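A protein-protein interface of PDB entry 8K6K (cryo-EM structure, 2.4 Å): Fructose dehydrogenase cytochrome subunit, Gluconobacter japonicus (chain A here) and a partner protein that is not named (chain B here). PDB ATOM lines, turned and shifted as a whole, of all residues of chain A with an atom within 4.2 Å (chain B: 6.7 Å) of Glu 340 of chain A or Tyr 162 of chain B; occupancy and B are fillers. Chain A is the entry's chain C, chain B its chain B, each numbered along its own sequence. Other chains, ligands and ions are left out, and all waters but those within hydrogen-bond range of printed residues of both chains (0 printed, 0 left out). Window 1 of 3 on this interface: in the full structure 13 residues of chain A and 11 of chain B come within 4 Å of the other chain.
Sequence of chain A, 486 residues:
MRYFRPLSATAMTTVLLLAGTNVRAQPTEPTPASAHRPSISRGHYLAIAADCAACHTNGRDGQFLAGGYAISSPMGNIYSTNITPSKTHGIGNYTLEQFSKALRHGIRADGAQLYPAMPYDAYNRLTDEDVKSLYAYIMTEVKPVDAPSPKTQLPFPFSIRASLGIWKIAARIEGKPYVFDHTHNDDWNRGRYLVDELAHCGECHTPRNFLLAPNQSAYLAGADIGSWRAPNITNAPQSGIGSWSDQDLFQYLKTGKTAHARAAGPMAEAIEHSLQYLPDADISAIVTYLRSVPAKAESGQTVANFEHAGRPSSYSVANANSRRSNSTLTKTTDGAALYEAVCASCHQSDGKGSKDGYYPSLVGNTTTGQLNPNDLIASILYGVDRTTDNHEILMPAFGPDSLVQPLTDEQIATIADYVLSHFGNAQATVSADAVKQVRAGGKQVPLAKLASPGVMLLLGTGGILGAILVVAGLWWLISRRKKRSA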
ATOM      1  N   TYR A 315       1.489 -19.898  -2.374  1.00  0.00           N
ATOM      2  CA  TYR A 315       2.729 -19.968  -1.620  1.00  0.00           C
ATOM      3  C   TYR A 315       3.875 -20.349  -2.555  1.00  0.00           C
ATOM      4  O   TYR A 315       3.729 -20.374  -3.780  1.00  0.00           O
ATOM      5  CB  TYR A 315       2.592 -20.953  -0.459  1.00  0.00           C
ATOM      6  CG  TYR A 315       2.792 -22.411  -0.810  1.00  0.00           C
ATOM      7  CD1 TYR A 315       2.210 -22.971  -1.938  1.00  0.00           C
ATOM      8  CD2 TYR A 315       3.565 -23.229   0.000  1.00  0.00           C
ATOM      9  CE1 TYR A 315       2.405 -24.297  -2.254  1.00  0.00           C
ATOM     10  CE2 TYR A 315       3.762 -24.554  -0.305  1.00  0.00           C
ATOM     11  CZ  TYR A 315       3.180 -25.084  -1.432  1.00  0.00           C
ATOM     12  OH  TYR A 315       3.373 -26.411  -1.737  1.00  0.00           O
ATOM     13  N   ALA A 336       0.628 -18.102   3.790  1.00  0.00           N
ATOM     14  CA  ALA A 336       0.429 -19.005   2.664  1.00  0.00           C
ATOM     15  C   ALA A 336       0.942 -20.402   2.981  1.00  0.00           C
ATOM     16  O   ALA A 336       0.283 -21.400   2.670  1.00  0.00           O
ATOM     17  CB  ALA A 336       1.120 -18.447   1.423  1.00  0.00           C
ATOM     18  N   ALA A 337       2.116 -20.492   3.609  1.00  0.00           N
ATOM     19  CA  ALA A 337       2.667 -21.793   3.971  1.00  0.00           C
ATOM     20  C   ALA A 337       1.787 -22.502   4.990  1.00  0.00           C
ATOM     21  O   ALA A 337       1.561 -23.713   4.890  1.00  0.00           O
ATOM     22  CB  ALA A 337       4.086 -21.630   4.510  1.00  0.00           C
ATOM     23  N   LEU A 338       1.288 -21.767   5.985  1.00  0.00           N
ATOM     24  CA  LEU A 338       0.412 -22.372   6.981  1.00  0.00           C
ATOM     25  C   LEU A 338      -0.883 -22.861   6.351  1.00  0.00           C
ATOM     26  O   LEU A 338      -1.355 -23.962   6.658  1.00  0.00           O
ATOM     27  CB  LEU A 338       0.119 -21.373   8.099  1.00  0.00           C
ATOM     28  CG  LEU A 338       1.167 -21.243   9.199  1.00  0.00           C
ATOM     29  CD1 LEU A 338       0.850 -20.059  10.092  1.00  0.00           C
ATOM     30  CD2 LEU A 338       1.246 -22.521  10.009  1.00  0.00           C
ATOM     31  N   TYR A 339      -1.472 -22.059   5.461  1.00  0.00           N
ATOM     32  CA  TYR A 339      -2.689 -22.489   4.783  1.00  0.00           C
ATOM     33  C   TYR A 339      -2.437 -23.729   3.941  1.00  0.00           C
ATOM     34  O   TYR A 339      -3.264 -24.646   3.910  1.00  0.00           O
ATOM     35  CB  TYR A 339      -3.243 -21.361   3.914  1.00  0.00           C
ATOM     36  CG  TYR A 339      -4.330 -21.815   2.967  1.00  0.00           C
ATOM     37  CD1 TYR A 339      -5.643 -21.925   3.394  1.00  0.00           C
ATOM     38  CD2 TYR A 339      -4.042 -22.142   1.650  1.00  0.00           C
ATOM     39  CE1 TYR A 339      -6.636 -22.347   2.538  1.00  0.00           C
ATOM     40  CE2 TYR A 339      -5.028 -22.564   0.791  1.00  0.00           C
ATOM     41  CZ  TYR A 339      -6.323 -22.664   1.239  1.00  0.00           C
ATOM     42  OH  TYR A 339      -7.310 -23.082   0.381  1.00  0.00           O
ATOM     43  N   GLU A 340      -1.302 -23.774   3.241  1.00  0.00           N
ATOM     44  CA  GLU A 340      -0.998 -24.939   2.423  1.00  0.00           C
ATOM     45  C   GLU A 340      -0.802 -26.183   3.278  1.00  0.00           C
ATOM     46  O   GLU A 340      -1.292 -27.264   2.936  1.00  0.00           O
ATOM     47  CB  GLU A 340       0.239 -24.681   1.569  1.00  0.00           C
ATOM     48  CG  GLU A 340       0.481 -25.755   0.534  1.00  0.00           C
ATOM     49  CD  GLU A 340      -0.312 -25.526  -0.732  1.00  0.00           C
ATOM     50  OE1 GLU A 340      -0.947 -24.460  -0.852  1.00  0.00           O
ATOM     51  OE2 GLU A 340      -0.299 -26.411  -1.610  1.00  0.00           O
ATOM     52  N   ALA A 341      -0.088 -26.050   4.394  1.00  0.00           N
ATOM     53  CA  ALA A 341       0.185 -27.210   5.233  1.00  0.00           C
ATOM     54  C   ALA A 341      -1.079 -27.719   5.911  1.00  0.00           C
ATOM     55  O   ALA A 341      -1.285 -28.933   6.015  1.00  0.00           O
ATOM     56  CB  ALA A 341       1.250 -26.867   6.272  1.00  0.00           C
ATOM     57  N   VAL A 342      -1.940 -26.817   6.371  1.00  0.00           N
ATOM     58  CA  VAL A 342      -3.083 -27.193   7.190  1.00  0.00           C
ATOM     59  C   VAL A 342      -4.350 -27.362   6.363  1.00  0.00           C
ATOM     60  O   VAL A 342      -5.092 -28.324   6.559  1.00  0.00           O
ATOM     61  CB  VAL A 342      -3.294 -26.161   8.319  1.00  0.00           C
ATOM     62  CG1 VAL A 342      -4.396 -26.620   9.252  1.00  0.00           C
ATOM     63  CG2 VAL A 342      -2.007 -25.944   9.086  1.00  0.00           C
ATOM     64  N   ALA A 344      -4.804 -26.729   2.630  1.00  0.00           N
ATOM     65  CA  ALA A 344      -4.822 -26.893   1.181  1.00  0.00           C
ATOM     66  C   ALA A 344      -5.206 -28.299   0.742  1.00  0.00           C
ATOM     67  O   ALA A 344      -5.515 -28.497  -0.436  1.00  0.00           O
ATOM     68  CB  ALA A 344      -3.468 -26.533   0.580  1.00  0.00           C
ATOM     69  N   SER A 345      -5.191 -29.276   1.650  1.00  0.00           N
ATOM     70  CA  SER A 345      -5.494 -30.647   1.254  1.00  0.00           C
ATOM     71  C   SER A 345      -6.919 -30.776   0.734  1.00  0.00           C
ATOM     72  O   SER A 345      -7.156 -31.423  -0.292  1.00  0.00           O
ATOM     73  CB  SER A 345      -5.265 -31.594   2.429  1.00  0.00           C
ATOM     74  OG  SER A 345      -5.507 -32.935   2.049  1.00  0.00           O
ATOM     75  N   GLN A 348      -8.442 -26.583  -2.257  1.00  0.00           N
ATOM     76  CA  GLN A 348      -7.218 -26.659  -3.038  1.00  0.00           C
ATOM     77  C   GLN A 348      -6.363 -25.406  -2.837  1.00  0.00           C
ATOM     78  O   GLN A 348      -6.780 -24.420  -2.227  1.00  0.00           O
ATOM     79  CB  GLN A 348      -7.550 -26.866  -4.512  1.00  0.00           C
ATOM     80  CG  GLN A 348      -8.367 -28.115  -4.775  1.00  0.00           C
ATOM     81  CD  GLN A 348      -7.891 -29.303  -3.963  1.00  0.00           C
ATOM     82  OE1 GLN A 348      -6.778 -29.790  -4.150  1.00  0.00           O
ATOM     83  NE2 GLN A 348      -8.734 -29.775  -3.057  1.00  0.00           N
ATOM     84  N   SER A 349      -5.134 -25.464  -3.358  1.00  0.00           N
ATOM     85  CA  SER A 349      -4.185 -24.374  -3.155  1.00  0.00           C
ATOM     86  C   SER A 349      -4.717 -23.051  -3.688  1.00  0.00           C
ATOM     87  O   SER A 349      -4.389 -21.990  -3.147  1.00  0.00           O
ATOM     88  CB  SER A 349      -2.850 -24.709  -3.817  1.00  0.00           C
ATOM     89  OG  SER A 349      -1.779 -24.079  -3.140  1.00  0.00           O
ATOM     90  N   PHE B 144       5.764 -29.272  -6.297  1.00  0.00           N
ATOM     91  CA  PHE B 144       4.935 -30.438  -6.035  1.00  0.00           C
ATOM     92  C   PHE B 144       3.488 -30.053  -6.293  1.00  0.00           C
ATOM     93  O   PHE B 144       3.070 -28.939  -5.966  1.00  0.00           O
ATOM     94  CB  PHE B 144       5.096 -30.953  -4.605  1.00  0.00           C
ATOM     95  CG  PHE B 144       4.274 -32.172  -4.308  1.00  0.00           C
ATOM     96  CD1 PHE B 144       4.473 -33.343  -5.013  1.00  0.00           C
ATOM     97  CD2 PHE B 144       3.300 -32.146  -3.329  1.00  0.00           C
ATOM     98  CE1 PHE B 144       3.719 -34.464  -4.745  1.00  0.00           C
ATOM     99  CE2 PHE B 144       2.545 -33.265  -3.058  1.00  0.00           C
ATOM    100  CZ  PHE B 144       2.756 -34.424  -3.766  1.00  0.00           C
ATOM    101  N   GLU B 145       2.745 -30.969  -6.919  1.00  0.00           N
ATOM    102  CA  GLU B 145       1.360 -30.768  -7.342  1.00  0.00           C
ATOM    103  C   GLU B 145       1.309 -29.811  -8.527  1.00  0.00           C
ATOM    104  O   GLU B 145       0.257 -29.630  -9.147  1.00  0.00           O
ATOM    105  CB  GLU B 145       0.486 -30.259  -6.192  1.00  0.00           C
ATOM    106  CG  GLU B 145      -1.003 -30.458  -6.407  1.00  0.00           C
ATOM    107  CD  GLU B 145      -1.824 -29.270  -5.957  1.00  0.00           C
ATOM    108  OE1 GLU B 145      -1.234 -28.201  -5.703  1.00  0.00           O
ATOM    109  OE2 GLU B 145      -3.060 -29.405  -5.858  1.00  0.00           O
ATOM    110  N   ARG B 154      -3.437 -36.466 -13.788  1.00  0.00           N
ATOM    111  CA  ARG B 154      -4.191 -35.699 -12.805  1.00  0.00           C
ATOM    112  C   ARG B 154      -5.680 -36.002 -12.873  1.00  0.00           C
ATOM    113  O   ARG B 154      -6.364 -35.984 -11.845  1.00  0.00           O
ATOM    114  CB  ARG B 154      -3.956 -34.204 -13.009  1.00  0.00           C
ATOM    115  CG  ARG B 154      -2.907 -33.613 -12.101  1.00  0.00           C
ATOM    116  CD  ARG B 154      -3.079 -32.116 -11.976  1.00  0.00           C
ATOM    117  NE  ARG B 154      -3.731 -31.747 -10.727  1.00  0.00           N
ATOM    118  CZ  ARG B 154      -3.392 -30.697  -9.993  1.00  0.00           C
ATOM    119  NH1 ARG B 154      -2.412 -29.889 -10.355  1.00  0.00           N
ATOM    120  NH2 ARG B 154      -4.055 -30.453  -8.866  1.00  0.00           N
ATOM    121  N   VAL B 158      -4.656 -39.484  -7.987  1.00  0.00           N
ATOM    122  CA  VAL B 158      -4.554 -38.415  -7.006  1.00  0.00           C
ATOM    123  C   VAL B 158      -3.092 -38.036  -6.818  1.00  0.00           C
ATOM    124  O   VAL B 158      -2.205 -38.896  -6.796  1.00  0.00           O
ATOM    125  CB  VAL B 158      -5.193 -38.855  -5.676  1.00  0.00           C
ATOM    126  CG1 VAL B 158      -4.599 -40.170  -5.212  1.00  0.00           C
ATOM    127  CG2 VAL B 158      -5.014 -37.795  -4.611  1.00  0.00           C
ATOM    128  N   ILE B 159      -2.829 -36.738  -6.704  1.00  0.00           N
ATOM    129  CA  ILE B 159      -1.554 -36.276  -6.171  1.00  0.00           C
ATOM    130  C   ILE B 159      -1.698 -36.379  -4.659  1.00  0.00           C
ATOM    131  O   ILE B 159      -2.510 -35.652  -4.070  1.00  0.00           O
ATOM    132  CB  ILE B 159      -1.226 -34.852  -6.640  1.00  0.00           C
ATOM    133  CG1 ILE B 159      -1.269 -34.781  -8.165  1.00  0.00           C
ATOM    134  CG2 ILE B 159       0.134 -34.424  -6.130  1.00  0.00           C
ATOM    135  CD1 ILE B 159      -1.052 -33.403  -8.718  1.00  0.00           C
ATOM    136  N   PRO B 160      -0.927 -37.247  -3.996  1.00  0.00           N
ATOM    137  CA  PRO B 160      -1.341 -37.779  -2.688  1.00  0.00           C
ATOM    138  C   PRO B 160      -1.841 -36.784  -1.649  1.00  0.00           C
ATOM    139  O   PRO B 160      -3.006 -36.861  -1.251  1.00  0.00           O
ATOM    140  CB  PRO B 160      -0.072 -38.483  -2.207  1.00  0.00           C
ATOM    141  CG  PRO B 160       0.535 -38.991  -3.464  1.00  0.00           C
ATOM    142  CD  PRO B 160       0.253 -37.953  -4.522  1.00  0.00           C
ATOM    143  N   THR B 161      -1.029 -35.825  -1.219  1.00  0.00           N
ATOM    144  CA  THR B 161      -1.498 -35.023  -0.093  1.00  0.00           C
ATOM    145  C   THR B 161      -2.574 -34.012  -0.474  1.00  0.00           C
ATOM    146  O   THR B 161      -2.982 -33.226   0.385  1.00  0.00           O
ATOM    147  CB  THR B 161      -0.326 -34.303   0.567  1.00  0.00           C
ATOM    148  OG1 THR B 161       0.576 -33.838  -0.441  1.00  0.00           O
ATOM    149  CG2 THR B 161       0.403 -35.243   1.508  1.00  0.00           C
ATOM    150  N   TYR B 162      -3.044 -34.009  -1.717  1.00  0.00           N
ATOM    151  CA  TYR B 162      -4.095 -33.110  -2.167  1.00  0.00           C
ATOM    152  C   TYR B 162      -5.271 -33.932  -2.664  1.00  0.00           C
ATOM    153  O   TYR B 162      -5.104 -34.809  -3.516  1.00  0.00           O
ATOM    154  CB  TYR B 162      -3.583 -32.177  -3.263  1.00  0.00           C
ATOM    155  CG  TYR B 162      -2.511 -31.236  -2.781  1.00  0.00           C
ATOM    156  CD1 TYR B 162      -2.838 -30.014  -2.216  1.00  0.00           C
ATOM    157  CD2 TYR B 162      -1.171 -31.572  -2.881  1.00  0.00           C
ATOM    158  CE1 TYR B 162      -1.865 -29.152  -1.773  1.00  0.00           C
ATOM    159  CE2 TYR B 162      -0.189 -30.716  -2.440  1.00  0.00           C
ATOM    160  CZ  TYR B 162      -0.540 -29.507  -1.886  1.00  0.00           C
ATOM    161  OH  TYR B 162       0.437 -28.648  -1.444  1.00  0.00           O
ATOM    162  N   ALA B 163      -6.455 -33.640  -2.140  1.00  0.00           N
ATOM    163  CA  ALA B 163      -7.616 -34.485  -2.369  1.00  0.00           C
ATOM    164  C   ALA B 163      -8.167 -34.321  -3.778  1.00  0.00           C
ATOM    165  O   ALA B 163      -8.176 -33.221  -4.336  1.00  0.00           O
ATOM    166  CB  ALA B 163      -8.708 -34.165  -1.352  1.00  0.00           C
ATOM    167  N   HIS B 164      -8.624 -35.431  -4.348  1.00  0.00           N
ATOM    168  CA  HIS B 164      -9.502 -35.408  -5.505  1.00  0.00           C
ATOM    169  C   HIS B 164     -10.914 -35.047  -5.044  1.00  0.00           C
ATOM    170  O   HIS B 164     -11.178 -34.861  -3.854  1.00  0.00           O
ATOM    171  CB  HIS B 164      -9.473 -36.758  -6.215  1.00  0.00           C
ATOM    172  CG  HIS B 164      -8.925 -36.707  -7.606  1.00  0.00           C
ATOM    173  ND1 HIS B 164      -9.651 -37.116  -8.704  1.00  0.00           N
ATOM    174  CD2 HIS B 164      -7.720 -36.310  -8.078  1.00  0.00           C
ATOM    175  CE1 HIS B 164      -8.918 -36.967  -9.793  1.00  0.00           C
ATOM    176  NE2 HIS B 164      -7.743 -36.478  -9.441  1.00  0.00           N
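The backbone carbonyl oxygen of Thr 161 of chain B sits at hydrogen-bond distance from the side-chain hydroxyl of Ser 345 of chain A (3.0 Å). The backbone carbonyl oxygen (O) of Ser 345 of chain A is in hydrogen-bond range of the backbone NH (N) of Ala 163 of chain B (3.0 Å). OE2 of Glu 340 of chain A sits close to OH of Tyr 162 of chain B, 2.4 Å away.
The backbone NH of Ala 344 of chain A lies within hydrogen-bond range of the backbone carbonyl oxygen of Tyr 339 of chain A (2.9 Å). OH of Tyr 339 of chain A is in hydrogen-bond range of O of Gln 348 of chain A, 3.0 Å away. OG of Ser 349 of chain A lies within hydrogen-bond range of OE1 of Glu 340 of chain A.
Among the printed residues, pairs that only touch across the chains: Tyr 315 of chain A with Tyr 162 of chain B (3.7 Å), Ala 344 of chain A with Tyr 162 of chain B (3.6 Å), Ser 345 of chain A with Tyr 162 of chain B (3.9 Å) and Gln 348 of chain A with Ala 163 of chain B (3.7 Å).
Printed residues of chain B within 4 Å of Tyr 315 of chain A: Tyr 162 (3.7 Å). Leu 338 of chain A touches none of the printed residues of chain B. Tyr 339 of chain A touches none of the printed residues of chain B. Of chain B, only Tyr 162 comes within 4 Å of Glu 340 of chain A. Of the printed residues of chain B, Ala 344 of chain A touches Tyr 162 (3.6 Å). Of the printed residues of chain B, Gln 348 of chain A touches Ala 163. Printed residues of chain A within 4 Å of Thr 161 of chain B: Ser 345 (3.0 Å). Of chain A, only Tyr 315, Glu 340, Ala 344 and Ser 345 come within 4 Å of Tyr 162 of chain B. The nearest residue of chain A that does not touch Tyr 162 of chain B is Gln 348 of chain A (4.1 Å).
Of the 12 printed residues of chain A, 5 touch a printed residue of chain B. Of the 10 printed residues of chain B, 3 touch a printed residue of chain A. Printed residues of chain B that touch a printed residue of chain A: Thr 161, Tyr 162 and Ala 163. Hydrophobic or aromatic side chains of chain B that line the printed part of chain A: Tyr 162 and Ala 163. Among the printed residues, 7 pairs touch across the chains. Among the printed residues, no Asp or Glu carboxylate lies within 4 Å of a Lys or Arg side-chain nitrogen of the other chain.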
